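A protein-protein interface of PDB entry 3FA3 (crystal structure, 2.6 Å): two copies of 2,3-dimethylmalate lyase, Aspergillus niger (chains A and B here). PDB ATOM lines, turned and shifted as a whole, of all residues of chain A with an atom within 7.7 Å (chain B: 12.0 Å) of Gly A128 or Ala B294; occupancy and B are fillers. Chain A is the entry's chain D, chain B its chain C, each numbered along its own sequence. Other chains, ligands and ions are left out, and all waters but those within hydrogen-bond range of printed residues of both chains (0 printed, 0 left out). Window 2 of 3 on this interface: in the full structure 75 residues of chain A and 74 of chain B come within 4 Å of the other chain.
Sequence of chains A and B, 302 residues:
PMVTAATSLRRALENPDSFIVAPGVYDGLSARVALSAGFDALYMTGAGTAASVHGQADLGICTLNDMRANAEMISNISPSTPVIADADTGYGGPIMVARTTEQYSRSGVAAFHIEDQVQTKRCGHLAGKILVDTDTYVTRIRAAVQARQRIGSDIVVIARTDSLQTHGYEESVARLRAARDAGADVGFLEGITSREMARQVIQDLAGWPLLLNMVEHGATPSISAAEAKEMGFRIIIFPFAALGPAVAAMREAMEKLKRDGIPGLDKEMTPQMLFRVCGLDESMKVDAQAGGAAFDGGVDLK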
ATOM      1  N   GLN A 117       8.179  17.649  14.927  1.00  0.00           N
ATOM      2  CA  GLN A 117       9.446  17.335  14.254  1.00  0.00           C
ATOM      3  C   GLN A 117       9.454  17.602  12.742  1.00  0.00           C
ATOM      4  O   GLN A 117       8.447  18.015  12.178  1.00  0.00           O
ATOM      5  CB  GLN A 117       9.810  15.880  14.489  1.00  0.00           C
ATOM      6  CG  GLN A 117      10.287  15.492  15.858  1.00  0.00           C
ATOM      7  CD  GLN A 117      10.605  14.021  15.881  1.00  0.00           C
ATOM      8  OE1 GLN A 117      11.511  13.503  15.129  1.00  0.00           O
ATOM      9  NE2 GLN A 117       9.855  13.305  16.733  1.00  0.00           N
ATOM     10  N   THR A 120      10.781  13.713   8.297  1.00  0.00           N
ATOM     11  CA  THR A 120      11.586  12.476   8.537  1.00  0.00           C
ATOM     12  C   THR A 120      11.890  12.394  10.052  1.00  0.00           C
ATOM     13  O   THR A 120      13.016  12.641  10.553  1.00  0.00           O
ATOM     14  CB  THR A 120      12.812  12.334   7.603  1.00  0.00           C
ATOM     15  OG1 THR A 120      13.616  13.506   7.660  1.00  0.00           O
ATOM     16  CG2 THR A 120      12.372  12.167   6.201  1.00  0.00           C
ATOM     17  N   ARG A 122      11.652  10.969  14.173  1.00  0.00           N
ATOM     18  CA  ARG A 122      12.421   9.982  14.943  1.00  0.00           C
ATOM     19  C   ARG A 122      11.621   9.472  16.146  1.00  0.00           C
ATOM     20  O   ARG A 122      10.793  10.195  16.663  1.00  0.00           O
ATOM     21  CB  ARG A 122      13.627  10.724  15.451  1.00  0.00           C
ATOM     22  CG  ARG A 122      14.601   9.949  16.270  1.00  0.00           C
ATOM     23  CD  ARG A 122      15.940  10.718  16.350  1.00  0.00           C
ATOM     24  NE  ARG A 122      16.137  11.598  15.156  1.00  0.00           N
ATOM     25  CZ  ARG A 122      17.335  11.951  14.677  1.00  0.00           C
ATOM     26  NH1 ARG A 122      17.411  12.736  13.619  1.00  0.00           N
ATOM     27  NH2 ARG A 122      18.440  11.489  15.261  1.00  0.00           N
ATOM     28  N   CYS A 123      11.841   8.251  16.624  1.00  0.00           N
ATOM     29  CA  CYS A 123      11.224   7.921  17.895  1.00  0.00           C
ATOM     30  C   CYS A 123      11.562   8.998  18.879  1.00  0.00           C
ATOM     31  O   CYS A 123      12.689   9.385  18.970  1.00  0.00           O
ATOM     32  CB  CYS A 123      11.691   6.589  18.441  1.00  0.00           C
ATOM     33  SG  CYS A 123      11.189   6.414  20.180  1.00  0.00           S
ATOM     34  N   GLY A 124      10.556   9.460  19.612  1.00  0.00           N
ATOM     35  CA  GLY A 124      10.680  10.485  20.653  1.00  0.00           C
ATOM     36  C   GLY A 124      11.757  10.232  21.718  1.00  0.00           C
ATOM     37  O   GLY A 124      12.453  11.181  22.142  1.00  0.00           O
ATOM     38  N   HIS A 125      11.915   8.980  22.157  1.00  0.00           N
ATOM     39  CA  HIS A 125      12.967   8.618  23.130  1.00  0.00           C
ATOM     40  C   HIS A 125      14.339   8.393  22.485  1.00  0.00           C
ATOM     41  O   HIS A 125      15.190   7.738  23.077  1.00  0.00           O
ATOM     42  CB  HIS A 125      12.534   7.429  24.006  1.00  0.00           C
ATOM     43  CG  HIS A 125      11.452   7.786  24.982  1.00  0.00           C
ATOM     44  ND1 HIS A 125      11.714   8.074  26.312  1.00  0.00           N
ATOM     45  CD2 HIS A 125      10.113   7.974  24.807  1.00  0.00           C
ATOM     46  CE1 HIS A 125      10.581   8.411  26.919  1.00  0.00           C
ATOM     47  NE2 HIS A 125       9.594   8.358  26.030  1.00  0.00           N
ATOM     48  N   LEU A 126      14.555   8.950  21.282  1.00  0.00           N
ATOM     49  CA  LEU A 126      15.890   8.913  20.639  1.00  0.00           C
ATOM     50  C   LEU A 126      16.630  10.251  20.659  1.00  0.00           C
ATOM     51  O   LEU A 126      16.010  11.320  20.569  1.00  0.00           O
ATOM     52  CB  LEU A 126      15.825   8.384  19.207  1.00  0.00           C
ATOM     53  CG  LEU A 126      15.384   6.920  19.077  1.00  0.00           C
ATOM     54  CD1 LEU A 126      15.279   6.562  17.635  1.00  0.00           C
ATOM     55  CD2 LEU A 126      16.434   6.071  19.750  1.00  0.00           C
ATOM     56  N   ALA A 127      17.953  10.196  20.838  1.00  0.00           N
ATOM     57  CA  ALA A 127      18.766  11.422  20.808  1.00  0.00           C
ATOM     58  C   ALA A 127      18.844  12.100  19.402  1.00  0.00           C
ATOM     59  O   ALA A 127      18.677  11.419  18.345  1.00  0.00           O
ATOM     60  CB  ALA A 127      20.188  11.165  21.414  1.00  0.00           C
ATOM     61  N   GLY A 128      19.049  13.425  19.408  1.00  0.00           N
ATOM     62  CA  GLY A 128      19.438  14.176  18.194  1.00  0.00           C
ATOM     63  C   GLY A 128      18.305  14.552  17.245  1.00  0.00           C
ATOM     64  O   GLY A 128      18.517  14.752  16.028  1.00  0.00           O
ATOM     65  N   LYS A 129      17.112  14.627  17.825  1.00  0.00           N
ATOM     66  CA  LYS A 129      15.916  14.991  17.143  1.00  0.00           C
ATOM     67  C   LYS A 129      16.039  16.348  16.396  1.00  0.00           C
ATOM     68  O   LYS A 129      16.835  17.259  16.802  1.00  0.00           O
ATOM     69  CB  LYS A 129      14.789  15.059  18.165  1.00  0.00           C
ATOM     70  CG  LYS A 129      14.336  13.713  18.746  1.00  0.00           C
ATOM     71  CD  LYS A 129      12.927  13.826  19.383  1.00  0.00           C
ATOM     72  CE  LYS A 129      12.931  14.322  20.761  1.00  0.00           C
ATOM     73  NZ  LYS A 129      11.708  13.821  21.383  1.00  0.00           N
ATOM     74  N   ILE A 130      15.242  16.495  15.322  1.00  0.00           N
ATOM     75  CA  ILE A 130      15.229  17.769  14.555  1.00  0.00           C
ATOM     76  C   ILE A 130      13.837  18.335  14.431  1.00  0.00           C
ATOM     77  O   ILE A 130      12.938  17.669  13.970  1.00  0.00           O
ATOM     78  CB  ILE A 130      15.866  17.634  13.132  1.00  0.00           C
ATOM     79  CG1 ILE A 130      17.135  16.743  13.195  1.00  0.00           C
ATOM     80  CG2 ILE A 130      16.092  19.044  12.481  1.00  0.00           C
ATOM     81  CD1 ILE A 130      17.433  15.969  11.886  1.00  0.00           C
ATOM     82  N   LEU A 131      13.660  19.586  14.839  1.00  0.00           N
ATOM     83  CA  LEU A 131      12.317  20.101  14.946  1.00  0.00           C
ATOM     84  C   LEU A 131      12.009  21.153  13.901  1.00  0.00           C
ATOM     85  O   LEU A 131      12.906  21.643  13.192  1.00  0.00           O
ATOM     86  CB  LEU A 131      12.109  20.675  16.331  1.00  0.00           C
ATOM     87  CG  LEU A 131      12.322  19.685  17.474  1.00  0.00           C
ATOM     88  CD1 LEU A 131      12.773  20.486  18.631  1.00  0.00           C
ATOM     89  CD2 LEU A 131      11.055  18.914  17.847  1.00  0.00           C
ATOM     90  N   GLN A 165      13.719  17.883  24.699  1.00  0.00           N
ATOM     91  CA  GLN A 165      15.084  17.391  24.541  1.00  0.00           C
ATOM     92  C   GLN A 165      15.983  18.433  23.962  1.00  0.00           C
ATOM     93  O   GLN A 165      17.042  18.695  24.492  1.00  0.00           O
ATOM     94  CB  GLN A 165      15.148  16.137  23.657  1.00  0.00           C
ATOM     95  CG  GLN A 165      16.549  15.575  23.406  1.00  0.00           C
ATOM     96  CD  GLN A 165      16.505  14.542  22.295  1.00  0.00           C
ATOM     97  OE1 GLN A 165      16.848  14.806  21.125  1.00  0.00           O
ATOM     98  NE2 GLN A 165      16.017  13.349  22.644  1.00  0.00           N
ATOM     99  N   THR A 166      15.562  19.003  22.842  1.00  0.00           N
ATOM    100  CA  THR A 166      16.422  19.920  22.095  1.00  0.00           C
ATOM    101  C   THR A 166      16.387  21.271  22.745  1.00  0.00           C
ATOM    102  O   THR A 166      17.468  21.792  23.069  1.00  0.00           O
ATOM    103  CB  THR A 166      15.987  20.126  20.627  1.00  0.00           C
ATOM    104  OG1 THR A 166      15.135  19.049  20.209  1.00  0.00           O
ATOM    105  CG2 THR A 166      17.243  20.191  19.727  1.00  0.00           C
ATOM    106  N   GLN B 272      15.664   1.886  21.764  1.00  0.00           N
ATOM    107  CA  GLN B 272      16.853   1.534  20.967  1.00  0.00           C
ATOM    108  C   GLN B 272      17.031   0.024  20.827  1.00  0.00           C
ATOM    109  O   GLN B 272      17.188  -0.493  19.709  1.00  0.00           O
ATOM    110  CB  GLN B 272      18.130   2.131  21.565  1.00  0.00           C
ATOM    111  CG  GLN B 272      18.248   3.651  21.366  1.00  0.00           C
ATOM    112  CD  GLN B 272      17.670   4.462  22.573  1.00  0.00           C
ATOM    113  OE1 GLN B 272      16.768   3.994  23.311  1.00  0.00           O
ATOM    114  NE2 GLN B 272      18.198   5.682  22.775  1.00  0.00           N
ATOM    115  N   ARG B 276      16.891  -1.601  17.136  1.00  0.00           N
ATOM    116  CA  ARG B 276      18.093  -2.258  16.681  1.00  0.00           C
ATOM    117  C   ARG B 276      17.810  -3.646  16.134  1.00  0.00           C
ATOM    118  O   ARG B 276      18.394  -4.025  15.139  1.00  0.00           O
ATOM    119  CB  ARG B 276      19.196  -2.205  17.720  1.00  0.00           C
ATOM    120  CG  ARG B 276      20.263  -1.202  17.277  1.00  0.00           C
ATOM    121  CD  ARG B 276      21.505  -1.215  18.116  1.00  0.00           C
ATOM    122  NE  ARG B 276      21.524  -0.147  19.130  1.00  0.00           N
ATOM    123  CZ  ARG B 276      21.875   1.130  18.931  1.00  0.00           C
ATOM    124  NH1 ARG B 276      22.248   1.590  17.739  1.00  0.00           N
ATOM    125  NH2 ARG B 276      21.858   1.964  19.955  1.00  0.00           N
ATOM    126  N   LEU B 280      17.961  -0.663  12.718  1.00  0.00           N
ATOM    127  CA  LEU B 280      18.332   0.715  13.086  1.00  0.00           C
ATOM    128  C   LEU B 280      19.788   1.107  12.832  1.00  0.00           C
ATOM    129  O   LEU B 280      20.049   2.107  12.155  1.00  0.00           O
ATOM    130  CB  LEU B 280      17.928   1.025  14.529  1.00  0.00           C
ATOM    131  CG  LEU B 280      18.397   2.401  15.046  1.00  0.00           C
ATOM    132  CD1 LEU B 280      17.381   3.528  14.803  1.00  0.00           C
ATOM    133  CD2 LEU B 280      18.815   2.321  16.523  1.00  0.00           C
ATOM    134  N   ASP B 281      20.732   0.354  13.389  1.00  0.00           N
ATOM    135  CA  ASP B 281      22.127   0.442  12.963  1.00  0.00           C
ATOM    136  C   ASP B 281      22.307   0.561  11.441  1.00  0.00           C
ATOM    137  O   ASP B 281      23.014   1.464  10.986  1.00  0.00           O
ATOM    138  CB  ASP B 281      22.917  -0.746  13.520  1.00  0.00           C
ATOM    139  CG  ASP B 281      23.144  -0.641  15.059  1.00  0.00           C
ATOM    140  OD1 ASP B 281      23.523  -1.675  15.726  1.00  0.00           O
ATOM    141  OD2 ASP B 281      22.936   0.488  15.584  1.00  0.00           O
ATOM    142  N   GLU B 282      21.668  -0.313  10.661  1.00  0.00           N
ATOM    143  CA  GLU B 282      21.871  -0.303   9.172  1.00  0.00           C
ATOM    144  C   GLU B 282      21.208   0.921   8.456  1.00  0.00           C
ATOM    145  O   GLU B 282      21.768   1.515   7.508  1.00  0.00           O
ATOM    146  CB  GLU B 282      21.435  -1.634   8.510  1.00  0.00           C
ATOM    147  CG  GLU B 282      21.418  -1.638   6.941  1.00  0.00           C
ATOM    148  CD  GLU B 282      22.840  -1.487   6.228  1.00  0.00           C
ATOM    149  OE1 GLU B 282      22.892  -0.908   5.104  1.00  0.00           O
ATOM    150  OE2 GLU B 282      23.907  -1.953   6.758  1.00  0.00           O
ATOM    151  N   SER B 283      20.019   1.278   8.951  1.00  0.00           N
ATOM    152  CA  SER B 283      19.313   2.409   8.480  1.00  0.00           C
ATOM    153  C   SER B 283      20.192   3.611   8.796  1.00  0.00           C
ATOM    154  O   SER B 283      20.321   4.531   7.967  1.00  0.00           O
ATOM    155  CB  SER B 283      17.975   2.493   9.195  1.00  0.00           C
ATOM    156  OG  SER B 283      17.050   1.539   8.689  1.00  0.00           O
ATOM    157  N   MET B 284      20.834   3.609   9.967  1.00  0.00           N
ATOM    158  CA  MET B 284      21.657   4.762  10.347  1.00  0.00           C
ATOM    159  C   MET B 284      22.899   4.901   9.490  1.00  0.00           C
ATOM    160  O   MET B 284      23.426   5.976   9.403  1.00  0.00           O
ATOM    161  CB  MET B 284      22.024   4.731  11.820  1.00  0.00           C
ATOM    162  CG  MET B 284      20.942   5.238  12.746  1.00  0.00           C
ATOM    163  SD  MET B 284      21.446   5.361  14.494  1.00  0.00           S
ATOM    164  CE  MET B 284      22.444   3.882  14.790  1.00  0.00           C
ATOM    165  N   LYS B 285      23.360   3.809   8.871  1.00  0.00           N
ATOM    166  CA  LYS B 285      24.551   3.831   8.019  1.00  0.00           C
ATOM    167  C   LYS B 285      24.201   4.398   6.688  1.00  0.00           C
ATOM    168  O   LYS B 285      24.957   5.184   6.139  1.00  0.00           O
ATOM    169  CB  LYS B 285      25.170   2.449   7.804  1.00  0.00           C
ATOM    170  CG  LYS B 285      26.200   2.138   8.839  1.00  0.00           C
ATOM    171  CD  LYS B 285      26.818   0.668   8.784  1.00  0.00           C
ATOM    172  CE  LYS B 285      27.074   0.154  10.271  1.00  0.00           C
ATOM    173  NZ  LYS B 285      28.088  -0.917  10.448  1.00  0.00           N
ATOM    174  N   VAL B 286      23.050   4.002   6.155  1.00  0.00           N
ATOM    175  CA  VAL B 286      22.631   4.430   4.828  1.00  0.00           C
ATOM    176  C   VAL B 286      22.713   5.952   4.740  1.00  0.00           C
ATOM    177  O   VAL B 286      23.248   6.520   3.778  1.00  0.00           O
ATOM    178  CB  VAL B 286      21.202   3.947   4.540  1.00  0.00           C
ATOM    179  CG1 VAL B 286      20.593   4.702   3.296  1.00  0.00           C
ATOM    180  CG2 VAL B 286      21.183   2.387   4.423  1.00  0.00           C
ATOM    181  N   ASP B 287      22.172   6.577   5.786  1.00  0.00           N
ATOM    182  CA  ASP B 287      22.141   8.028   5.957  1.00  0.00           C
ATOM    183  C   ASP B 287      23.566   8.597   6.004  1.00  0.00           C
ATOM    184  O   ASP B 287      23.912   9.506   5.219  1.00  0.00           O
ATOM    185  CB  ASP B 287      21.343   8.401   7.226  1.00  0.00           C
ATOM    186  CG  ASP B 287      21.206   9.910   7.411  1.00  0.00           C
ATOM    187  OD1 ASP B 287      20.273  10.533   6.871  1.00  0.00           O
ATOM    188  OD2 ASP B 287      22.070  10.483   8.100  1.00  0.00           O
ATOM    189  N   ALA B 288      24.386   8.028   6.893  1.00  0.00           N
ATOM    190  CA  ALA B 288      25.717   8.545   7.169  1.00  0.00           C
ATOM    191  C   ALA B 288      26.568   8.454   5.914  1.00  0.00           C
ATOM    192  O   ALA B 288      27.314   9.369   5.561  1.00  0.00           O
ATOM    193  CB  ALA B 288      26.331   7.765   8.280  1.00  0.00           C
ATOM    194  N   GLN B 289      26.418   7.319   5.241  1.00  0.00           N
ATOM    195  CA  GLN B 289      27.065   7.069   3.988  1.00  0.00           C
ATOM    196  C   GLN B 289      26.706   8.081   2.959  1.00  0.00           C
ATOM    197  O   GLN B 289      27.542   8.383   2.138  1.00  0.00           O
ATOM    198  CB  GLN B 289      26.648   5.708   3.470  1.00  0.00           C
ATOM    199  CG  GLN B 289      27.763   4.666   3.365  1.00  0.00           C
ATOM    200  CD  GLN B 289      27.299   3.249   3.669  1.00  0.00           C
ATOM    201  OE1 GLN B 289      26.105   2.967   3.774  1.00  0.00           O
ATOM    202  NE2 GLN B 289      28.252   2.362   3.853  1.00  0.00           N
ATOM    203  N   ALA B 290      25.509   8.646   3.000  1.00  0.00           N
ATOM    204  CA  ALA B 290      24.971   9.251   1.779  1.00  0.00           C
ATOM    205  C   ALA B 290      25.281  10.671   1.337  1.00  0.00           C
ATOM    206  O   ALA B 290      25.071  10.927   0.186  1.00  0.00           O
ATOM    207  CB  ALA B 290      23.468   8.993   1.657  1.00  0.00           C
ATOM    208  N   GLY B 291      25.757  11.533   2.229  1.00  0.00           N
ATOM    209  CA  GLY B 291      25.956  11.162   3.617  1.00  0.00           C
ATOM    210  C   GLY B 291      25.316  12.146   4.578  1.00  0.00           C
ATOM    211  O   GLY B 291      25.653  13.329   4.586  1.00  0.00           O
ATOM    212  N   GLY B 292      24.390  11.651   5.392  1.00  0.00           N
ATOM    213  CA  GLY B 292      23.489  12.513   6.134  1.00  0.00           C
ATOM    214  C   GLY B 292      24.012  12.842   7.520  1.00  0.00           C
ATOM    215  O   GLY B 292      24.996  12.261   7.976  1.00  0.00           O
ATOM    216  N   ALA B 293      23.357  13.776   8.169  1.00  0.00           N
ATOM    217  CA  ALA B 293      23.812  14.289   9.416  1.00  0.00           C
ATOM    218  C   ALA B 293      22.846  13.930  10.464  1.00  0.00           C
ATOM    219  O   ALA B 293      23.024  14.266  11.574  1.00  0.00           O
ATOM    220  CB  ALA B 293      23.925  15.710   9.335  1.00  0.00           C
ATOM    221  N   ALA B 294      21.802  13.242  10.074  1.00  0.00           N
ATOM    222  CA  ALA B 294      20.597  13.174  10.831  1.00  0.00           C
ATOM    223  C   ALA B 294      20.881  12.485  12.116  1.00  0.00           C
ATOM    224  O   ALA B 294      20.209  12.658  13.079  1.00  0.00           O
ATOM    225  CB  ALA B 294      19.594  12.430  10.079  1.00  0.00           C
ATOM    226  N   PHE B 295      21.895  11.672  12.100  1.00  0.00           N
ATOM    227  CA  PHE B 295      21.967  10.635  13.055  1.00  0.00           C
ATOM    228  C   PHE B 295      23.156  10.829  13.875  1.00  0.00           C
ATOM    229  O   PHE B 295      23.759   9.885  14.283  1.00  0.00           O
ATOM    230  CB  PHE B 295      21.965   9.289  12.378  1.00  0.00           C
ATOM    231  CG  PHE B 295      20.625   8.851  12.006  1.00  0.00           C
ATOM    232  CD1 PHE B 295      20.373   8.327  10.800  1.00  0.00           C
ATOM    233  CD2 PHE B 295      19.613   9.010  12.880  1.00  0.00           C
ATOM    234  CE1 PHE B 295      19.153   7.974  10.506  1.00  0.00           C
ATOM    235  CE2 PHE B 295      18.427   8.669  12.590  1.00  0.00           C
ATOM    236  CZ  PHE B 295      18.169   8.153  11.421  1.00  0.00           C
ATOM    237  N   ASP B 296      23.510  12.084  14.126  1.00  0.00           N
ATOM    238  CA  ASP B 296      24.899  12.454  14.377  1.00  0.00           C
ATOM    239  C   ASP B 296      25.201  12.478  15.872  1.00  0.00           C
ATOM    240  O   ASP B 296      24.674  13.313  16.608  1.00  0.00           O
ATOM    241  CB  ASP B 296      25.212  13.816  13.755  1.00  0.00           C
ATOM    242  CG  ASP B 296      26.527  13.823  13.002  1.00  0.00           C
ATOM    243  OD1 ASP B 296      27.452  13.091  13.411  1.00  0.00           O
ATOM    244  OD2 ASP B 296      26.636  14.561  11.999  1.00  0.00           O
ATOM    245  N   GLY B 297      26.053  11.559  16.313  1.00  0.00           N
ATOM    246  CA  GLY B 297      26.200  11.273  17.728  1.00  0.00           C
ATOM    247  C   GLY B 297      25.273  10.169  18.197  1.00  0.00           C
ATOM    248  O   GLY B 297      24.764  10.206  19.317  1.00  0.00           O
ATOM    249  N   GLY B 298      25.055   9.181  17.335  1.00  0.00           N
ATOM    250  CA  GLY B 298      23.868   8.368  17.402  1.00  0.00           C
ATOM    251  C   GLY B 298      22.672   8.854  18.180  1.00  0.00           C
ATOM    252  O   GLY B 298      22.378  10.010  18.306  1.00  0.00           O
ATOM    253  N   VAL B 299      21.974   7.888  18.708  1.00  0.00           N
ATOM    254  CA  VAL B 299      20.633   8.078  19.225  1.00  0.00           C
ATOM    255  C   VAL B 299      20.474   7.632  20.656  1.00  0.00           C
ATOM    256  O   VAL B 299      19.380   7.431  21.108  1.00  0.00           O
ATOM    257  CB  VAL B 299      19.605   7.304  18.350  1.00  0.00           C
ATOM    258  CG1 VAL B 299      19.380   8.002  16.951  1.00  0.00           C
ATOM    259  CG2 VAL B 299      20.081   5.817  18.190  1.00  0.00           C
ATOM    260  N   ASP B 300      21.564   7.477  21.381  1.00  0.00           N
ATOM    261  CA  ASP B 300      21.466   6.945  22.732  1.00  0.00           C
ATOM    262  C   ASP B 300      21.312   8.045  23.727  1.00  0.00           C
ATOM    263  O   ASP B 300      21.674   9.194  23.438  1.00  0.00           O
ATOM    264  CB  ASP B 300      22.621   6.010  23.033  1.00  0.00           C
ATOM    265  CG  ASP B 300      22.578   4.796  22.105  1.00  0.00           C
ATOM    266  OD1 ASP B 300      21.570   4.003  22.175  1.00  0.00           O
ATOM    267  OD2 ASP B 300      23.499   4.698  21.246  1.00  0.00           O
ATOM    268  N   LEU B 301      20.727   7.737  24.879  1.00  0.00           N
ATOM    269  CA  LEU B 301      20.206   8.838  25.643  1.00  0.00           C
ATOM    270  C   LEU B 301      21.200   9.139  26.797  1.00  0.00           C
ATOM    271  O   LEU B 301      22.131  10.010  26.591  1.00  0.00           O
ATOM    272  CB  LEU B 301      18.734   8.556  26.034  1.00  0.00           C
ATOM    273  CG  LEU B 301      17.665   9.654  25.771  1.00  0.00           C
ATOM    274  CD1 LEU B 301      17.827  10.333  24.417  1.00  0.00           C
ATOM    275  CD2 LEU B 301      16.228   9.097  25.894  1.00  0.00           C
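The backbone carbonyl oxygen (O) of Ala B294 is in hydrogen-bond range of the guanidinium group (NH1) of Arg A122 (2.9 Å).
The backbone carbonyl oxygen of Val B299 sits at hydrogen-bond distance from the backbone NH of Ala A127, 3.1 Å away.
The side-chain amide nitrogen of Gln B272 sits at hydrogen-bond distance from the backbone carbonyl oxygen of Val B299 (2.7 Å).
The side-chain carboxylate of Asp B300 is in salt-bridge range of the guanidinium group of Arg B276 (3.0 Å).
N of Ala B294 is in hydrogen-bond range of OD2 of Asp B287, at 3.4 Å.
NH1 of Arg A122 lies close to O of Gly A128, at 3.3 Å.
The side-chain sulfur (SG) of Cys A123 lies close to the backbone NH (N) of His A125.
The side-chain amide nitrogen (NE2) of Gln A165 is in hydrogen-bond range of the backbone carbonyl oxygen (O) of Leu A126 (2.9 Å).
Among the printed residues, pairs that only touch across the chains: Arg A122 with Phe B295, Arg A122 with Val B299, His A125 with Gln B272, His A125 with Leu B301, Leu A126 with Gln B272, Leu A126 with Val B299, Leu A126 with Leu B301, Ala A127 with Gly B298, Ala A127 with Asp B300, Ala A127 with Leu B301, Gly A128 with Ala B294 and Gln A165 with Leu B301.
Of the printed residues of chain B, Gly A128 touches Ala B294 (3.99 Å).
Of the printed residues of chain A, Ala B294 touches Arg A122 and Gly A128.
Of chain B, only Gly B298, Val B299, Asp B300 and Leu B301 come within 4 Å of Ala A127.
Lys A129 touches none of the printed residues of chain B.
No residue of chain B comes within 4 Å of Ile A130.
No residue of chain A comes within 4 Å of Ala B293.
Printed residues of chain A within 4 Å of Val B299: Arg A122, Leu A126 and Ala A127.
Of the printed residues of chain A, Gln B272 touches His A125 and Leu A126.
Of the printed residues of chain A, Leu B301 touches His A125, Leu A126, Ala A127 and Gln A165.
Of the printed residues of chain A, Phe B295 touches Arg A122 (3.6 Å).
Printed residues of chain A within 4 Å of Gly B298: Ala A127.
Gln B289 touches none of the printed residues of chain A.
Ser B283 touches none of the printed residues of chain A.
The nearest printed residue of chain B that does not touch Gly A128 is Gly B298 (4.9 Å).
The nearest printed residue of chain A that does not touch Ala B294 is Ile A130 (4.4 Å).
Hydrophobic or aromatic side chains of chain A within 4 Å of the printed part of chain B: Leu A126 and Ala A127.
Of the 24 printed residues of chain B, 7 touch a printed residue of chain A.
Among the printed residues, 14 pairs touch across the chains.
Among the printed residues, no Asp or Glu carboxylate lies within 4 Å of a Lys or Arg side-chain nitrogen of the other chain.
No position is printed for both chains.
Of the 14 pairs that touch across the chains among the printed residues, none has its exchanged pair printed and touching as well.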
